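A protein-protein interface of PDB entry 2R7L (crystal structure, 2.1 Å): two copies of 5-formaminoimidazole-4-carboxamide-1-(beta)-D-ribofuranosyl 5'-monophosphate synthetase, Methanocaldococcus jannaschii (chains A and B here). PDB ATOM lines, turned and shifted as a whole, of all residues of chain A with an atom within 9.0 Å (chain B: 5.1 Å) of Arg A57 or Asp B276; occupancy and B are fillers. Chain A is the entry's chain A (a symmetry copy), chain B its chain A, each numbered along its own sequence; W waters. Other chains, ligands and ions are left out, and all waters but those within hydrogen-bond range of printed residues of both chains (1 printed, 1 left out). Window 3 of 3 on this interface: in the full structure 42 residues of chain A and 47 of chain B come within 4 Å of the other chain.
Printed residues of chain A that touch a printed residue of chain B: Val A53, Pro A54, Arg A57 and Phe A58.
Hydrophobic or aromatic side chains of chain A that line the printed part of chain B: Val A53, Pro A54 and Phe A58.
Of the 13 printed residues of chain B, 5 touch a printed residue of chain A.
Among the printed residues, 9 pairs touch across the chains.
The guanidinium group (NH1) of Arg A57 lies within hydrogen-bond range of the backbone carbonyl oxygen (O) of Val B220 (3.0 Å).
The side-chain carboxylate of Asp B276 is in salt-bridge range of the guanidinium group of Arg A57.
Of the printed residues of chain B, Pro A54 touches Phe B272.
Arg A57 touches five residues of chain B.
Printed residues of chain B within 4 Å of Phe A58: Phe B272 (3.8 Å) and Tyr B332 (3.3 Å).
Printed residues of chain A within 4 Å of Glu B219: Arg A57.
Of chain A, only Arg A57 comes within 4 Å of Val B220.
No residue of chain A comes within 4 Å of Gly B275.
Of the printed residues of chain A, Tyr B332 touches Arg A57 (3.2 Å) and Phe A58 (3.3 Å).
The nearest printed residue of chain B that does not touch Arg A57 is Gly B275 (6.3 Å).
The nearest residue of chain A that does not touch Asp B276 is Val A53 (4.8 Å).
The nearest printed residue of chain B that does not touch Pro A54 is Tyr B332 (6.9 Å).
CG1 of Val A53 touches CG of Phe B272 (3.8 Å).
Phe B272 touches Pro A54.
OE1 of Glu B219 touches CD of Arg A57, at 3.4 Å.
Arg A57 touches Phe B272.
O of Arg A57 touches CE1 of Tyr B332 (3.2 Å).
Phe A58 touches Phe B272 (CE2 to CZ, 3.8 Å).
Tyr B332 touches Phe A58.
No position is printed for both chains.
Water W1 lies within hydrogen-bond range of the backbone carbonyl oxygen (O) of Arg A57 (2.5 Å) and the side-chain carboxylate (OE1) of Glu B219 (2.8 Å).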
ATOM      1  N   LEU A  30      26.802  15.907   0.424  1.00  0.00           N
ATOM      2  CA  LEU A  30      27.176  14.489   0.497  1.00  0.00           C
ATOM      3  C   LEU A  30      28.098  14.044  -0.633  1.00  0.00           C
ATOM      4  O   LEU A  30      29.080  13.354  -0.377  1.00  0.00           O
ATOM      5  CB  LEU A  30      25.953  13.583   0.577  1.00  0.00           C
ATOM      6  CG  LEU A  30      25.294  13.530   1.958  1.00  0.00           C
ATOM      7  CD1 LEU A  30      24.041  12.672   1.926  1.00  0.00           C
ATOM      8  CD2 LEU A  30      26.268  13.021   2.987  1.00  0.00           C
ATOM      9  N   GLY A  50      21.946  18.157  15.822  1.00  0.00           N
ATOM     10  CA  GLY A  50      20.656  17.825  15.237  1.00  0.00           C
ATOM     11  C   GLY A  50      20.680  17.561  13.739  1.00  0.00           C
ATOM     12  O   GLY A  50      19.786  16.894  13.214  1.00  0.00           O
ATOM     13  N   ASP A  52      23.853  16.663  11.995  1.00  0.00           N
ATOM     14  CA  ASP A  52      25.197  16.170  11.674  1.00  0.00           C
ATOM     15  C   ASP A  52      25.247  14.676  11.376  1.00  0.00           C
ATOM     16  O   ASP A  52      26.201  14.196  10.762  1.00  0.00           O
ATOM     17  CB  ASP A  52      26.207  16.540  12.778  1.00  0.00           C
ATOM     18  CG  ASP A  52      25.822  15.994  14.141  1.00  0.00           C
ATOM     19  OD1 ASP A  52      24.642  15.652  14.347  1.00  0.00           O
ATOM     20  OD2 ASP A  52      26.707  15.915  15.018  1.00  0.00           O
ATOM     21  N   VAL A  53      24.218  13.953  11.803  1.00  0.00           N
ATOM     22  CA  VAL A  53      24.171  12.498  11.657  1.00  0.00           C
ATOM     23  C   VAL A  53      24.451  11.951  10.249  1.00  0.00           C
ATOM     24  O   VAL A  53      25.201  10.989  10.106  1.00  0.00           O
ATOM     25  CB  VAL A  53      22.845  11.916  12.184  1.00  0.00           C
ATOM     26  CG1 VAL A  53      22.731  10.443  11.829  1.00  0.00           C
ATOM     27  CG2 VAL A  53      22.759  12.099  13.684  1.00  0.00           C
ATOM     28  N   PRO A  54      23.848  12.549   9.206  1.00  0.00           N
ATOM     29  CA  PRO A  54      24.062  11.994   7.868  1.00  0.00           C
ATOM     30  C   PRO A  54      25.531  12.053   7.452  1.00  0.00           C
ATOM     31  O   PRO A  54      26.030  11.143   6.790  1.00  0.00           O
ATOM     32  CB  PRO A  54      23.229  12.919   6.967  1.00  0.00           C
ATOM     33  CG  PRO A  54      22.237  13.570   7.884  1.00  0.00           C
ATOM     34  CD  PRO A  54      22.966  13.729   9.176  1.00  0.00           C
ATOM     35  N   TYR A  55      26.206  13.122   7.852  1.00  0.00           N
ATOM     36  CA  TYR A  55      27.603  13.364   7.502  1.00  0.00           C
ATOM     37  C   TYR A  55      28.554  12.524   8.338  1.00  0.00           C
ATOM     38  O   TYR A  55      29.673  12.234   7.917  1.00  0.00           O
ATOM     39  CB  TYR A  55      27.893  14.864   7.612  1.00  0.00           C
ATOM     40  CG  TYR A  55      26.855  15.584   6.807  1.00  0.00           C
ATOM     41  CD1 TYR A  55      26.972  15.659   5.430  1.00  0.00           C
ATOM     42  CD2 TYR A  55      25.701  16.093   7.403  1.00  0.00           C
ATOM     43  CE1 TYR A  55      26.005  16.257   4.667  1.00  0.00           C
ATOM     44  CE2 TYR A  55      24.719  16.701   6.636  1.00  0.00           C
ATOM     45  CZ  TYR A  55      24.882  16.778   5.266  1.00  0.00           C
ATOM     46  OH  TYR A  55      23.930  17.367   4.466  1.00  0.00           O
ATOM     47  N   LYS A  56      28.082  12.104   9.506  1.00  0.00           N
ATOM     48  CA  LYS A  56      28.863  11.246  10.375  1.00  0.00           C
ATOM     49  C   LYS A  56      28.731   9.797   9.952  1.00  0.00           C
ATOM     50  O   LYS A  56      29.722   9.074   9.861  1.00  0.00           O
ATOM     51  CB  LYS A  56      28.446  11.429  11.831  1.00  0.00           C
ATOM     52  CG  LYS A  56      28.811  12.802  12.382  1.00  0.00           C
ATOM     53  CD  LYS A  56      28.684  12.857  13.888  1.00  0.00           C
ATOM     54  CE  LYS A  56      27.297  12.459  14.334  1.00  0.00           C
ATOM     55  NZ  LYS A  56      27.162  12.534  15.816  1.00  0.00           N
ATOM     56  N   ARG A  57      27.507   9.370   9.674  1.00  0.00           N
ATOM     57  CA  ARG A  57      27.268   7.970   9.342  1.00  0.00           C
ATOM     58  C   ARG A  57      27.677   7.621   7.915  1.00  0.00           C
ATOM     59  O   ARG A  57      27.981   6.468   7.611  1.00  0.00           O
ATOM     60  CB  ARG A  57      25.813   7.587   9.615  1.00  0.00           C
ATOM     61  CG  ARG A  57      25.397   7.912  11.035  1.00  0.00           C
ATOM     62  CD  ARG A  57      24.388   6.931  11.586  1.00  0.00           C
ATOM     63  NE  ARG A  57      23.941   7.375  12.899  1.00  0.00           N
ATOM     64  CZ  ARG A  57      22.726   7.161  13.393  1.00  0.00           C
ATOM     65  NH1 ARG A  57      21.823   6.500  12.681  1.00  0.00           N
ATOM     66  NH2 ARG A  57      22.415   7.617  14.601  1.00  0.00           N
ATOM     67  N   PHE A  58      27.685   8.609   7.036  1.00  0.00           N
ATOM     68  CA  PHE A  58      28.153   8.364   5.676  1.00  0.00           C
ATOM     69  C   PHE A  58      29.679   8.515   5.590  1.00  0.00           C
ATOM     70  O   PHE A  58      30.275   8.192   4.568  1.00  0.00           O
ATOM     71  CB  PHE A  58      27.424   9.252   4.661  1.00  0.00           C
ATOM     72  CG  PHE A  58      26.066   8.722   4.239  1.00  0.00           C
ATOM     73  CD1 PHE A  58      25.937   7.447   3.699  1.00  0.00           C
ATOM     74  CD2 PHE A  58      24.925   9.506   4.359  1.00  0.00           C
ATOM     75  CE1 PHE A  58      24.700   6.960   3.301  1.00  0.00           C
ATOM     76  CE2 PHE A  58      23.676   9.021   3.955  1.00  0.00           C
ATOM     77  CZ  PHE A  58      23.567   7.749   3.423  1.00  0.00           C
ATOM     78  N   LYS A  59      30.293   9.003   6.672  1.00  0.00           N
ATOM     79  CA  LYS A  59      31.753   8.992   6.851  1.00  0.00           C
ATOM     80  C   LYS A  59      32.451   9.819   5.791  1.00  0.00           C
ATOM     81  O   LYS A  59      33.488   9.435   5.266  1.00  0.00           O
ATOM     82  CB  LYS A  59      32.297   7.557   6.836  1.00  0.00           C
ATOM     83  CG  LYS A  59      31.832   6.691   8.005  1.00  0.00           C
ATOM     84  CD  LYS A  59      32.365   7.225   9.324  1.00  0.00           C
ATOM     85  CE  LYS A  59      31.677   6.571  10.517  1.00  0.00           C
ATOM     86  NZ  LYS A  59      31.718   7.468  11.711  1.00  0.00           N
ATOM     87  N   VAL A  60      31.885  10.983   5.512  1.00  0.00           N
ATOM     88  CA  VAL A  60      32.206  11.721   4.314  1.00  0.00           C
ATOM     89  C   VAL A  60      33.004  12.979   4.647  1.00  0.00           C
ATOM     90  O   VAL A  60      33.582  13.622   3.770  1.00  0.00           O
ATOM     91  CB  VAL A  60      30.880  12.014   3.538  1.00  0.00           C
ATOM     92  CG1 VAL A  60      30.424  13.465   3.689  1.00  0.00           C
ATOM     93  CG2 VAL A  60      31.008  11.599   2.097  1.00  0.00           C
ATOM     94  N   ALA A  61      33.066  13.312   5.932  1.00  0.00           N
ATOM     95  CA  ALA A  61      33.774  14.513   6.349  1.00  0.00           C
ATOM     96  C   ALA A  61      34.882  14.182   7.336  1.00  0.00           C
ATOM     97  O   ALA A  61      34.672  13.437   8.298  1.00  0.00           O
ATOM     98  CB  ALA A  61      32.810  15.528   6.946  1.00  0.00           C
ATOM     99  N   PHE A  64      34.838  18.402  11.240  1.00  0.00           N
ATOM    100  CA  PHE A  64      33.584  19.133  11.428  1.00  0.00           C
ATOM    101  C   PHE A  64      33.827  20.487  12.081  1.00  0.00           C
ATOM    102  O   PHE A  64      34.544  20.582  13.078  1.00  0.00           O
ATOM    103  CB  PHE A  64      32.614  18.335  12.294  1.00  0.00           C
ATOM    104  CG  PHE A  64      32.150  17.061  11.665  1.00  0.00           C
ATOM    105  CD1 PHE A  64      31.159  17.073  10.697  1.00  0.00           C
ATOM    106  CD2 PHE A  64      32.710  15.846  12.032  1.00  0.00           C
ATOM    107  CE1 PHE A  64      30.729  15.901  10.112  1.00  0.00           C
ATOM    108  CE2 PHE A  64      32.286  14.667  11.448  1.00  0.00           C
ATOM    109  CZ  PHE A  64      31.292  14.696  10.486  1.00  0.00           C
ATOM    110  N   GLU B 219      24.315   0.694  14.945  1.00  0.00           N
ATOM    111  CA  GLU B 219      24.154   1.850  14.078  1.00  0.00           C
ATOM    112  C   GLU B 219      23.043   1.611  13.069  1.00  0.00           C
ATOM    113  O   GLU B 219      22.896   0.504  12.538  1.00  0.00           O
ATOM    114  CB  GLU B 219      25.467   2.138  13.347  1.00  0.00           C
ATOM    115  CG  GLU B 219      25.535   3.494  12.658  1.00  0.00           C
ATOM    116  CD  GLU B 219      26.522   3.502  11.499  1.00  0.00           C
ATOM    117  OE1 GLU B 219      26.807   4.590  10.956  1.00  0.00           O
ATOM    118  OE2 GLU B 219      27.012   2.415  11.125  1.00  0.00           O
ATOM    119  N   VAL B 220      22.249   2.654  12.827  1.00  0.00           N
ATOM    120  CA  VAL B 220      21.227   2.634  11.780  1.00  0.00           C
ATOM    121  C   VAL B 220      21.821   3.276  10.533  1.00  0.00           C
ATOM    122  O   VAL B 220      22.276   4.416  10.571  1.00  0.00           O
ATOM    123  CB  VAL B 220      19.955   3.407  12.204  1.00  0.00           C
ATOM    124  CG1 VAL B 220      19.027   3.610  11.011  1.00  0.00           C
ATOM    125  CG2 VAL B 220      19.233   2.681  13.334  1.00  0.00           C
ATOM    126  N   PHE B 272      17.020  10.051   9.207  1.00  0.00           N
ATOM    127  CA  PHE B 272      17.845   9.298  10.157  1.00  0.00           C
ATOM    128  C   PHE B 272      17.193   9.238  11.538  1.00  0.00           C
ATOM    129  O   PHE B 272      17.152   8.173  12.166  1.00  0.00           O
ATOM    130  CB  PHE B 272      19.259   9.886  10.242  1.00  0.00           C
ATOM    131  CG  PHE B 272      20.206   9.351   9.196  1.00  0.00           C
ATOM    132  CD1 PHE B 272      20.539  10.111   8.086  1.00  0.00           C
ATOM    133  CD2 PHE B 272      20.756   8.083   9.323  1.00  0.00           C
ATOM    134  CE1 PHE B 272      21.408   9.619   7.117  1.00  0.00           C
ATOM    135  CE2 PHE B 272      21.619   7.581   8.359  1.00  0.00           C
ATOM    136  CZ  PHE B 272      21.951   8.351   7.259  1.00  0.00           C
ATOM    137  N   GLU B 273      16.672  10.375  12.002  1.00  0.00           N
ATOM    138  CA  GLU B 273      15.977  10.428  13.300  1.00  0.00           C
ATOM    139  C   GLU B 273      14.826   9.424  13.373  1.00  0.00           C
ATOM    140  O   GLU B 273      14.615   8.785  14.401  1.00  0.00           O
ATOM    141  CB  GLU B 273      15.469  11.843  13.593  1.00  0.00           C
ATOM    142  CG  GLU B 273      14.823  12.013  14.960  1.00  0.00           C
ATOM    143  CD  GLU B 273      15.827  11.941  16.102  1.00  0.00           C
ATOM    144  OE1 GLU B 273      16.920  12.532  15.976  1.00  0.00           O
ATOM    145  OE2 GLU B 273      15.522  11.298  17.131  1.00  0.00           O
ATOM    146  N   MET B 274      14.090   9.282  12.275  1.00  0.00           N
ATOM    147  CA  MET B 274      12.987   8.333  12.212  1.00  0.00           C
ATOM    148  C   MET B 274      13.488   6.918  12.384  1.00  0.00           C
ATOM    149  O   MET B 274      12.884   6.106  13.099  1.00  0.00           O
ATOM    150  CB  MET B 274      12.245   8.447  10.876  1.00  0.00           C
ATOM    151  CG  MET B 274      11.489   9.749  10.685  1.00  0.00           C
ATOM    152  SD  MET B 274      10.959   9.959   8.973  1.00  0.00           S
ATOM    153  CE  MET B 274       9.800   8.610   8.793  1.00  0.00           C
ATOM    154  N   GLY B 275      14.583   6.608  11.701  1.00  0.00           N
ATOM    155  CA  GLY B 275      15.217   5.295  11.837  1.00  0.00           C
ATOM    156  C   GLY B 275      15.731   5.077  13.252  1.00  0.00           C
ATOM    157  O   GLY B 275      15.526   4.020  13.840  1.00  0.00           O
ATOM    158  N   ASP B 276      16.378   6.091  13.812  1.00  0.00           N
ATOM    159  CA  ASP B 276      16.912   5.978  15.168  1.00  0.00           C
ATOM    160  C   ASP B 276      15.800   5.705  16.182  1.00  0.00           C
ATOM    161  O   ASP B 276      15.943   4.838  17.045  1.00  0.00           O
ATOM    162  CB  ASP B 276      17.705   7.234  15.544  1.00  0.00           C
ATOM    163  CG  ASP B 276      19.049   7.315  14.824  1.00  0.00           C
ATOM    164  OD1 ASP B 276      19.437   6.313  14.188  1.00  0.00           O
ATOM    165  OD2 ASP B 276      19.718   8.371  14.896  1.00  0.00           O
ATOM    166  N   LYS B 277      14.684   6.424  16.056  1.00  0.00           N
ATOM    167  CA  LYS B 277      13.560   6.276  16.986  1.00  0.00           C
ATOM    168  C   LYS B 277      12.888   4.920  16.881  1.00  0.00           C
ATOM    169  O   LYS B 277      12.611   4.282  17.894  1.00  0.00           O
ATOM    170  CB  LYS B 277      12.520   7.377  16.764  1.00  0.00           C
ATOM    171  CG  LYS B 277      12.960   8.755  17.197  1.00  0.00           C
ATOM    172  CD  LYS B 277      11.862   9.760  16.894  1.00  0.00           C
ATOM    173  CE  LYS B 277      12.200  11.139  17.414  1.00  0.00           C
ATOM    174  NZ  LYS B 277      11.110  12.093  17.086  1.00  0.00           N
ATOM    175  N   LEU B 278      12.614   4.479  15.660  1.00  0.00           N
ATOM    176  CA  LEU B 278      12.005   3.166  15.461  1.00  0.00           C
ATOM    177  C   LEU B 278      12.844   2.075  16.110  1.00  0.00           C
ATOM    178  O   LEU B 278      12.314   1.144  16.722  1.00  0.00           O
ATOM    179  CB  LEU B 278      11.818   2.865  13.969  1.00  0.00           C
ATOM    180  CG  LEU B 278      11.183   1.503  13.671  1.00  0.00           C
ATOM    181  CD1 LEU B 278       9.751   1.453  14.199  1.00  0.00           C
ATOM    182  CD2 LEU B 278      11.200   1.192  12.193  1.00  0.00           C
ATOM    183  N   VAL B 279      14.159   2.201  15.970  1.00  0.00           N
ATOM    184  CA  VAL B 279      15.102   1.216  16.491  1.00  0.00           C
ATOM    185  C   VAL B 279      15.162   1.229  18.022  1.00  0.00           C
ATOM    186  O   VAL B 279      15.116   0.177  18.656  1.00  0.00           O
ATOM    187  CB  VAL B 279      16.509   1.416  15.860  1.00  0.00           C
ATOM    188  CG1 VAL B 279      17.624   0.999  16.817  1.00  0.00           C
ATOM    189  CG2 VAL B 279      16.593   0.661  14.536  1.00  0.00           C
ATOM    190  N   ALA B 280      15.245   2.422  18.601  1.00  0.00           N
ATOM    191  CA  ALA B 280      15.302   2.576  20.050  1.00  0.00           C
ATOM    192  C   ALA B 280      14.057   2.025  20.743  1.00  0.00           C
ATOM    193  O   ALA B 280      14.159   1.418  21.807  1.00  0.00           O
ATOM    194  CB  ALA B 280      15.529   4.041  20.424  1.00  0.00           C
ATOM    195  N   LYS B 281      12.885   2.215  20.139  1.00  0.00           N
ATOM    196  CA  LYS B 281      11.654   1.710  20.740  1.00  0.00           C
ATOM    197  C   LYS B 281      11.491   0.209  20.547  1.00  0.00           C
ATOM    198  O   LYS B 281      11.023  -0.483  21.448  1.00  0.00           O
ATOM    199  CB  LYS B 281      10.416   2.451  20.212  1.00  0.00           C
ATOM    200  CG  LYS B 281       9.098   2.048  20.911  1.00  0.00           C
ATOM    201  CD  LYS B 281       9.093   2.383  22.415  1.00  0.00           C
ATOM    202  CE  LYS B 281       9.281   3.881  22.655  1.00  0.00           C
ATOM    203  NZ  LYS B 281       9.481   4.238  24.095  1.00  0.00           N
ATOM    204  N   TYR B 332      29.327   5.095   1.439  1.00  0.00           N
ATOM    205  CA  TYR B 332      30.141   4.440   2.462  1.00  0.00           C
ATOM    206  C   TYR B 332      31.565   4.119   2.003  1.00  0.00           C
ATOM    207  O   TYR B 332      32.537   4.486   2.673  1.00  0.00           O
ATOM    208  CB  TYR B 332      29.439   3.176   2.975  1.00  0.00           C
ATOM    209  CG  TYR B 332      28.102   3.488   3.616  1.00  0.00           C
ATOM    210  CD1 TYR B 332      28.035   4.117   4.853  1.00  0.00           C
ATOM    211  CD2 TYR B 332      26.905   3.195   2.965  1.00  0.00           C
ATOM    212  CE1 TYR B 332      26.819   4.424   5.438  1.00  0.00           C
ATOM    213  CE2 TYR B 332      25.677   3.504   3.541  1.00  0.00           C
ATOM    214  CZ  TYR B 332      25.645   4.115   4.780  1.00  0.00           C
ATOM    215  OH  TYR B 332      24.440   4.424   5.366  1.00  0.00           O
HETATM  216  O   HOH W   1      28.722   4.408   8.879  1.00  0.00           O
